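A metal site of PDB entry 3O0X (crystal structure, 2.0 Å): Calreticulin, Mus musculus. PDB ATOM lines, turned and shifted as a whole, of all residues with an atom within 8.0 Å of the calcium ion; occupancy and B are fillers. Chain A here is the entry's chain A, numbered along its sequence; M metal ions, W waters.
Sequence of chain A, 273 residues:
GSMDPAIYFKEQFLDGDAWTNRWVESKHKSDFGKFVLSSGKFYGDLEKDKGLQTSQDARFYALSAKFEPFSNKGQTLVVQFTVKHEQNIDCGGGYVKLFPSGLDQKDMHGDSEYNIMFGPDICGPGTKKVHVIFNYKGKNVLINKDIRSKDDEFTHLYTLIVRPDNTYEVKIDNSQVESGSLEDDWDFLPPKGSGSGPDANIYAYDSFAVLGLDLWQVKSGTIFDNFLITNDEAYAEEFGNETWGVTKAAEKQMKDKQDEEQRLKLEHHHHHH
NZ of Lys 50 is in salt-bridge range of OE2 of Glu 47 (3.4 Å).
The side-chain amino group of Lys 50 sits at hydrogen-bond distance from the backbone carbonyl oxygen of Leu 46, at 3.4 Å.
The side-chain amide nitrogen (NE2) of Gln 12 sits close to the side-chain amide nitrogen (ND2) of Asn 226 (3.3 Å).
The backbone NH (N) of Lys 48 is in hydrogen-bond range of the side-chain carboxylate (OD1) of Asp 45.
The backbone carbonyl oxygen (O) of Asp 225 is in hydrogen-bond range of the backbone NH (N) of Thr 82, 2.9 Å away.
Four residues have an atom within 4 Å of the calcium ion: Gln 12, Lys 48, Lys 50 and Asp 225.
Along chain A the residues within 4 Å of the calcium ion span positions 12 to 225.
The calcium ion is bound by water W2 (2.2 Å), the backbone carbonyl oxygen (O) of Lys 50 (2.3 Å), the backbone carbonyl oxygen (O) of Gln 12 (2.4 Å), water W1 (2.4 Å), the backbone carbonyl oxygen (O) of Lys 48 (2.5 Å), the side-chain carboxylate (OD2) of Asp 225 (2.5 Å) and the side-chain carboxylate (OD1) of Asp 225 (2.5 Å).
The calcium ion has seven donor atoms within binding distance.
Water W1 lies within hydrogen-bond range of the backbone carbonyl oxygen (O) of Glu 47 (2.7 Å) and the backbone carbonyl oxygen (O) of Phe 13 (2.9 Å).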
ATOM      1  N   GLU A  11      17.041  -9.552 -19.596  1.00  0.00           N
ATOM      2  CA  GLU A  11      17.270 -10.304 -18.354  1.00  0.00           C
ATOM      3  C   GLU A  11      18.404  -9.687 -17.546  1.00  0.00           C
ATOM      4  O   GLU A  11      19.552  -9.611 -18.016  1.00  0.00           O
ATOM      5  CB  GLU A  11      17.549 -11.776 -18.638  1.00  0.00           C
ATOM      6  CG  GLU A  11      17.759 -12.610 -17.364  1.00  0.00           C
ATOM      7  CD  GLU A  11      16.496 -12.753 -16.523  1.00  0.00           C
ATOM      8  OE1 GLU A  11      15.662 -13.617 -16.841  1.00  0.00           O
ATOM      9  OE2 GLU A  11      16.361 -12.011 -15.522  1.00  0.00           O
ATOM     10  N   GLN A  12      18.069  -9.232 -16.347  1.00  0.00           N
ATOM     11  CA  GLN A  12      19.010  -8.581 -15.445  1.00  0.00           C
ATOM     12  C   GLN A  12      19.128  -9.324 -14.131  1.00  0.00           C
ATOM     13  O   GLN A  12      19.932  -8.940 -13.286  1.00  0.00           O
ATOM     14  CB  GLN A  12      18.605  -7.135 -15.211  1.00  0.00           C
ATOM     15  CG  GLN A  12      18.710  -6.280 -16.469  1.00  0.00           C
ATOM     16  CD  GLN A  12      18.366  -4.850 -16.223  1.00  0.00           C
ATOM     17  OE1 GLN A  12      17.201  -4.464 -16.257  1.00  0.00           O
ATOM     18  NE2 GLN A  12      19.382  -4.021 -16.007  1.00  0.00           N
ATOM     19  N   PHE A  13      18.355 -10.394 -13.962  1.00  0.00           N
ATOM     20  CA  PHE A  13      18.370 -11.204 -12.735  1.00  0.00           C
ATOM     21  C   PHE A  13      18.234 -10.335 -11.477  1.00  0.00           C
ATOM     22  O   PHE A  13      19.046 -10.405 -10.541  1.00  0.00           O
ATOM     23  CB  PHE A  13      19.642 -12.062 -12.669  1.00  0.00           C
ATOM     24  CG  PHE A  13      19.903 -12.872 -13.913  1.00  0.00           C
ATOM     25  CD1 PHE A  13      19.220 -14.055 -14.137  1.00  0.00           C
ATOM     26  CD2 PHE A  13      20.828 -12.432 -14.863  1.00  0.00           C
ATOM     27  CE1 PHE A  13      19.444 -14.811 -15.291  1.00  0.00           C
ATOM     28  CE2 PHE A  13      21.073 -13.177 -16.020  1.00  0.00           C
ATOM     29  CZ  PHE A  13      20.362 -14.375 -16.234  1.00  0.00           C
ATOM     30  N   LEU A  14      17.189  -9.506 -11.456  1.00  0.00           N
ATOM     31  CA  LEU A  14      16.990  -8.552 -10.373  1.00  0.00           C
ATOM     32  C   LEU A  14      15.989  -9.024  -9.318  1.00  0.00           C
ATOM     33  O   LEU A  14      15.753  -8.322  -8.328  1.00  0.00           O
ATOM     34  CB  LEU A  14      16.576  -7.191 -10.949  1.00  0.00           C
ATOM     35  CG  LEU A  14      17.621  -6.366 -11.721  1.00  0.00           C
ATOM     36  CD1 LEU A  14      16.942  -5.290 -12.547  1.00  0.00           C
ATOM     37  CD2 LEU A  14      18.685  -5.749 -10.797  1.00  0.00           C
ATOM     38  N   ASP A  15      15.432 -10.226  -9.506  1.00  0.00           N
ATOM     39  CA  ASP A  15      14.361 -10.729  -8.618  1.00  0.00           C
ATOM     40  C   ASP A  15      14.687 -12.042  -7.866  1.00  0.00           C
ATOM     41  O   ASP A  15      13.778 -12.833  -7.571  1.00  0.00           O
ATOM     42  CB  ASP A  15      13.027 -10.833  -9.379  1.00  0.00           C
ATOM     43  CG  ASP A  15      13.070 -11.834 -10.538  1.00  0.00           C
ATOM     44  OD1 ASP A  15      14.150 -12.424 -10.813  1.00  0.00           O
ATOM     45  OD2 ASP A  15      12.017 -12.039 -11.184  1.00  0.00           O
ATOM     46  N   LEU A  37      22.971 -18.328  -9.436  1.00  0.00           N
ATOM     47  CA  LEU A  37      22.824 -16.876  -9.359  1.00  0.00           C
ATOM     48  C   LEU A  37      23.895 -16.298  -8.425  1.00  0.00           C
ATOM     49  O   LEU A  37      23.983 -16.668  -7.259  1.00  0.00           O
ATOM     50  CB  LEU A  37      21.421 -16.512  -8.863  1.00  0.00           C
ATOM     51  CG  LEU A  37      21.056 -15.027  -8.760  1.00  0.00           C
ATOM     52  CD1 LEU A  37      20.872 -14.394 -10.129  1.00  0.00           C
ATOM     53  CD2 LEU A  37      19.802 -14.884  -7.958  1.00  0.00           C
ATOM     54  N   SER A  38      24.704 -15.380  -8.956  1.00  0.00           N
ATOM     55  CA  SER A  38      25.867 -14.896  -8.196  1.00  0.00           C
ATOM     56  C   SER A  38      26.417 -13.581  -8.731  1.00  0.00           C
ATOM     57  O   SER A  38      26.459 -13.363  -9.945  1.00  0.00           O
ATOM     58  CB  SER A  38      26.958 -15.965  -8.202  1.00  0.00           C
ATOM     59  OG  SER A  38      28.138 -15.555  -7.519  1.00  0.00           O
ATOM     60  N   SER A  39      26.856 -12.707  -7.817  1.00  0.00           N
ATOM     61  CA  SER A  39      27.594 -11.512  -8.198  1.00  0.00           C
ATOM     62  C   SER A  39      29.120 -11.674  -8.034  1.00  0.00           C
ATOM     63  O   SER A  39      29.874 -10.728  -8.213  1.00  0.00           O
ATOM     64  CB  SER A  39      27.083 -10.268  -7.468  1.00  0.00           C
ATOM     65  OG  SER A  39      26.876 -10.539  -6.092  1.00  0.00           O
ATOM     66  N   ASP A  45      28.113  -3.703  -7.819  1.00  0.00           N
ATOM     67  CA  ASP A  45      27.023  -3.638  -6.826  1.00  0.00           C
ATOM     68  C   ASP A  45      26.560  -5.062  -6.507  1.00  0.00           C
ATOM     69  O   ASP A  45      26.311  -5.862  -7.416  1.00  0.00           O
ATOM     70  CB  ASP A  45      25.865  -2.800  -7.378  1.00  0.00           C
ATOM     71  CG  ASP A  45      24.744  -2.608  -6.374  1.00  0.00           C
ATOM     72  OD1 ASP A  45      23.836  -3.482  -6.293  1.00  0.00           O
ATOM     73  OD2 ASP A  45      24.761  -1.580  -5.674  1.00  0.00           O
ATOM     74  N   LEU A  46      26.468  -5.380  -5.211  1.00  0.00           N
ATOM     75  CA  LEU A  46      26.071  -6.736  -4.777  1.00  0.00           C
ATOM     76  C   LEU A  46      24.808  -7.244  -5.492  1.00  0.00           C
ATOM     77  O   LEU A  46      24.793  -8.383  -5.999  1.00  0.00           O
ATOM     78  CB  LEU A  46      25.891  -6.791  -3.252  1.00  0.00           C
ATOM     79  CG  LEU A  46      25.457  -8.134  -2.637  1.00  0.00           C
ATOM     80  CD1 LEU A  46      26.455  -9.247  -2.910  1.00  0.00           C
ATOM     81  CD2 LEU A  46      25.208  -7.994  -1.145  1.00  0.00           C
ATOM     82  N   GLU A  47      23.768  -6.420  -5.558  1.00  0.00           N
ATOM     83  CA  GLU A  47      22.509  -6.834  -6.179  1.00  0.00           C
ATOM     84  C   GLU A  47      22.443  -6.667  -7.694  1.00  0.00           C
ATOM     85  O   GLU A  47      22.025  -7.586  -8.385  1.00  0.00           O
ATOM     86  CB  GLU A  47      21.310  -6.153  -5.507  1.00  0.00           C
ATOM     87  CG  GLU A  47      20.404  -7.146  -4.800  1.00  0.00           C
ATOM     88  CD  GLU A  47      21.126  -7.920  -3.711  1.00  0.00           C
ATOM     89  OE1 GLU A  47      21.709  -7.277  -2.825  1.00  0.00           O
ATOM     90  OE2 GLU A  47      21.103  -9.175  -3.758  1.00  0.00           O
ATOM     91  N   LYS A  48      22.856  -5.514  -8.202  1.00  0.00           N
ATOM     92  CA  LYS A  48      22.799  -5.230  -9.633  1.00  0.00           C
ATOM     93  C   LYS A  48      23.647  -6.195 -10.466  1.00  0.00           C
ATOM     94  O   LYS A  48      23.301  -6.516 -11.614  1.00  0.00           O
ATOM     95  CB  LYS A  48      23.237  -3.798  -9.938  1.00  0.00           C
ATOM     96  CG  LYS A  48      22.276  -2.700  -9.495  1.00  0.00           C
ATOM     97  CD  LYS A  48      22.892  -1.332  -9.749  1.00  0.00           C
ATOM     98  CE  LYS A  48      21.875  -0.208  -9.571  1.00  0.00           C
ATOM     99  NZ  LYS A  48      22.557   1.114  -9.390  1.00  0.00           N
ATOM    100  N   ASP A  49      24.756  -6.670  -9.894  1.00  0.00           N
ATOM    101  CA  ASP A  49      25.687  -7.502 -10.671  1.00  0.00           C
ATOM    102  C   ASP A  49      25.477  -9.019 -10.507  1.00  0.00           C
ATOM    103  O   ASP A  49      26.306  -9.825 -10.915  1.00  0.00           O
ATOM    104  CB  ASP A  49      27.132  -7.069 -10.423  1.00  0.00           C
ATOM    105  CG  ASP A  49      27.404  -5.697 -10.996  1.00  0.00           C
ATOM    106  OD1 ASP A  49      27.055  -5.447 -12.169  1.00  0.00           O
ATOM    107  OD2 ASP A  49      27.958  -4.856 -10.269  1.00  0.00           O
ATOM    108  N   LYS A  50      24.331  -9.380  -9.927  1.00  0.00           N
ATOM    109  CA  LYS A  50      23.865 -10.754  -9.902  1.00  0.00           C
ATOM    110  C   LYS A  50      23.580 -11.184 -11.332  1.00  0.00           C
ATOM    111  O   LYS A  50      22.890 -10.479 -12.073  1.00  0.00           O
ATOM    112  CB  LYS A  50      22.575 -10.871  -9.080  1.00  0.00           C
ATOM    113  CG  LYS A  50      22.745 -10.835  -7.564  1.00  0.00           C
ATOM    114  CD  LYS A  50      23.075 -12.223  -7.019  1.00  0.00           C
ATOM    115  CE  LYS A  50      22.797 -12.322  -5.517  1.00  0.00           C
ATOM    116  NZ  LYS A  50      23.546 -11.322  -4.712  1.00  0.00           N
ATOM    117  N   GLY A  51      24.157 -12.321 -11.717  1.00  0.00           N
ATOM    118  CA  GLY A  51      23.936 -12.924 -13.030  1.00  0.00           C
ATOM    119  C   GLY A  51      24.129 -14.424 -12.951  1.00  0.00           C
ATOM    120  O   GLY A  51      24.288 -14.974 -11.857  1.00  0.00           O
ATOM    121  N   LEU A  52      24.155 -15.092 -14.098  1.00  0.00           N
ATOM    122  CA  LEU A  52      24.350 -16.544 -14.132  1.00  0.00           C
ATOM    123  C   LEU A  52      25.824 -16.905 -14.158  1.00  0.00           C
ATOM    124  O   LEU A  52      26.536 -16.540 -15.088  1.00  0.00           O
ATOM    125  CB  LEU A  52      23.676 -17.172 -15.348  1.00  0.00           C
ATOM    126  CG  LEU A  52      22.148 -17.110 -15.389  1.00  0.00           C
ATOM    127  CD1 LEU A  52      21.697 -17.603 -16.738  1.00  0.00           C
ATOM    128  CD2 LEU A  52      21.508 -17.894 -14.276  1.00  0.00           C
ATOM    129  N   THR A  82      26.548  -8.960 -21.000  1.00  0.00           N
ATOM    130  CA  THR A  82      27.872  -8.876 -20.379  1.00  0.00           C
ATOM    131  C   THR A  82      28.425 -10.261 -20.067  1.00  0.00           C
ATOM    132  O   THR A  82      27.665 -11.192 -19.751  1.00  0.00           O
ATOM    133  CB  THR A  82      27.883  -8.006 -19.099  1.00  0.00           C
ATOM    134  OG1 THR A  82      27.057  -8.592 -18.073  1.00  0.00           O
ATOM    135  CG2 THR A  82      27.413  -6.593 -19.410  1.00  0.00           C
ATOM    136  N   ILE A 223      30.510 -15.204 -15.311  1.00  0.00           N
ATOM    137  CA  ILE A 223      29.189 -14.659 -14.993  1.00  0.00           C
ATOM    138  C   ILE A 223      28.602 -13.905 -16.200  1.00  0.00           C
ATOM    139  O   ILE A 223      29.262 -13.030 -16.784  1.00  0.00           O
ATOM    140  CB  ILE A 223      29.214 -13.705 -13.763  1.00  0.00           C
ATOM    141  CG1 ILE A 223      30.024 -14.315 -12.609  1.00  0.00           C
ATOM    142  CG2 ILE A 223      27.757 -13.330 -13.305  1.00  0.00           C
ATOM    143  CD1 ILE A 223      30.130 -13.417 -11.362  1.00  0.00           C
ATOM    144  N   PHE A 224      27.371 -14.266 -16.572  1.00  0.00           N
ATOM    145  CA  PHE A 224      26.595 -13.583 -17.620  1.00  0.00           C
ATOM    146  C   PHE A 224      25.478 -12.728 -17.014  1.00  0.00           C
ATOM    147  O   PHE A 224      24.837 -13.142 -16.056  1.00  0.00           O
ATOM    148  CB  PHE A 224      25.953 -14.601 -18.565  1.00  0.00           C
ATOM    149  CG  PHE A 224      26.928 -15.572 -19.178  1.00  0.00           C
ATOM    150  CD1 PHE A 224      27.254 -16.749 -18.542  1.00  0.00           C
ATOM    151  CD2 PHE A 224      27.530 -15.274 -20.405  1.00  0.00           C
ATOM    152  CE1 PHE A 224      28.174 -17.656 -19.129  1.00  0.00           C
ATOM    153  CE2 PHE A 224      28.442 -16.148 -20.979  1.00  0.00           C
ATOM    154  CZ  PHE A 224      28.751 -17.348 -20.342  1.00  0.00           C
ATOM    155  N   ASP A 225      25.223 -11.556 -17.579  1.00  0.00           N
ATOM    156  CA  ASP A 225      24.240 -10.639 -17.009  1.00  0.00           C
ATOM    157  C   ASP A 225      23.741  -9.712 -18.101  1.00  0.00           C
ATOM    158  O   ASP A 225      24.339  -9.649 -19.180  1.00  0.00           O
ATOM    159  CB  ASP A 225      24.924  -9.813 -15.889  1.00  0.00           C
ATOM    160  CG  ASP A 225      23.941  -9.235 -14.881  1.00  0.00           C
ATOM    161  OD1 ASP A 225      22.706  -9.432 -15.018  1.00  0.00           O
ATOM    162  OD2 ASP A 225      24.426  -8.556 -13.939  1.00  0.00           O
ATOM    163  N   ASN A 226      22.640  -9.020 -17.823  1.00  0.00           N
ATOM    164  CA  ASN A 226      22.178  -7.906 -18.645  1.00  0.00           C
ATOM    165  C   ASN A 226      21.965  -8.275 -20.121  1.00  0.00           C
ATOM    166  O   ASN A 226      22.442  -7.588 -21.026  1.00  0.00           O
ATOM    167  CB  ASN A 226      23.133  -6.708 -18.503  1.00  0.00           C
ATOM    168  CG  ASN A 226      23.210  -6.210 -17.073  1.00  0.00           C
ATOM    169  OD1 ASN A 226      24.292  -6.053 -16.521  1.00  0.00           O
ATOM    170  ND2 ASN A 226      22.068  -5.951 -16.481  1.00  0.00           N
ATOM    171  N   PHE A 227      21.282  -9.397 -20.335  1.00  0.00           N
ATOM    172  CA  PHE A 227      20.875  -9.809 -21.681  1.00  0.00           C
ATOM    173  C   PHE A 227      19.865  -8.833 -22.238  1.00  0.00           C
ATOM    174  O   PHE A 227      18.931  -8.406 -21.522  1.00  0.00           O
ATOM    175  CB  PHE A 227      20.244 -11.188 -21.638  1.00  0.00           C
ATOM    176  CG  PHE A 227      21.197 -12.284 -21.280  1.00  0.00           C
ATOM    177  CD1 PHE A 227      21.995 -12.887 -22.256  1.00  0.00           C
ATOM    178  CD2 PHE A 227      21.308 -12.702 -19.964  1.00  0.00           C
ATOM    179  CE1 PHE A 227      22.879 -13.917 -21.929  1.00  0.00           C
ATOM    180  CE2 PHE A 227      22.196 -13.734 -19.621  1.00  0.00           C
ATOM    181  CZ  PHE A 227      22.976 -14.334 -20.610  1.00  0.00           C
ATOM    182  N   THR A 243      24.161  -0.250 -17.576  1.00  0.00           N
ATOM    183  CA  THR A 243      24.433  -1.544 -16.945  1.00  0.00           C
ATOM    184  C   THR A 243      25.932  -1.792 -16.801  1.00  0.00           C
ATOM    185  O   THR A 243      26.494  -1.571 -15.726  1.00  0.00           O
ATOM    186  CB  THR A 243      23.719  -2.715 -17.685  1.00  0.00           C
ATOM    187  OG1 THR A 243      24.068  -2.699 -19.063  1.00  0.00           O
ATOM    188  CG2 THR A 243      22.203  -2.598 -17.533  1.00  0.00           C
ATOM    189  N   THR A 247      28.741  -0.715 -13.876  1.00  0.00           N
ATOM    190  CA  THR A 247      29.500  -1.789 -13.215  1.00  0.00           C
ATOM    191  C   THR A 247      31.009  -1.572 -13.316  1.00  0.00           C
ATOM    192  O   THR A 247      31.756  -1.829 -12.352  1.00  0.00           O
ATOM    193  CB  THR A 247      29.160  -3.169 -13.877  1.00  0.00           C
ATOM    194  OG1 THR A 247      27.763  -3.455 -13.697  1.00  0.00           O
ATOM    195  CG2 THR A 247      29.986  -4.293 -13.279  1.00  0.00           C
HETATM  196 CA    CA M   1      22.216  -8.360 -12.829  1.00  0.00          CA
HETATM  197  O   HOH W   1      21.016  -8.293 -10.742  1.00  0.00           O
HETATM  198  O   HOH W   2      21.864  -6.409 -13.818  1.00  0.00           O
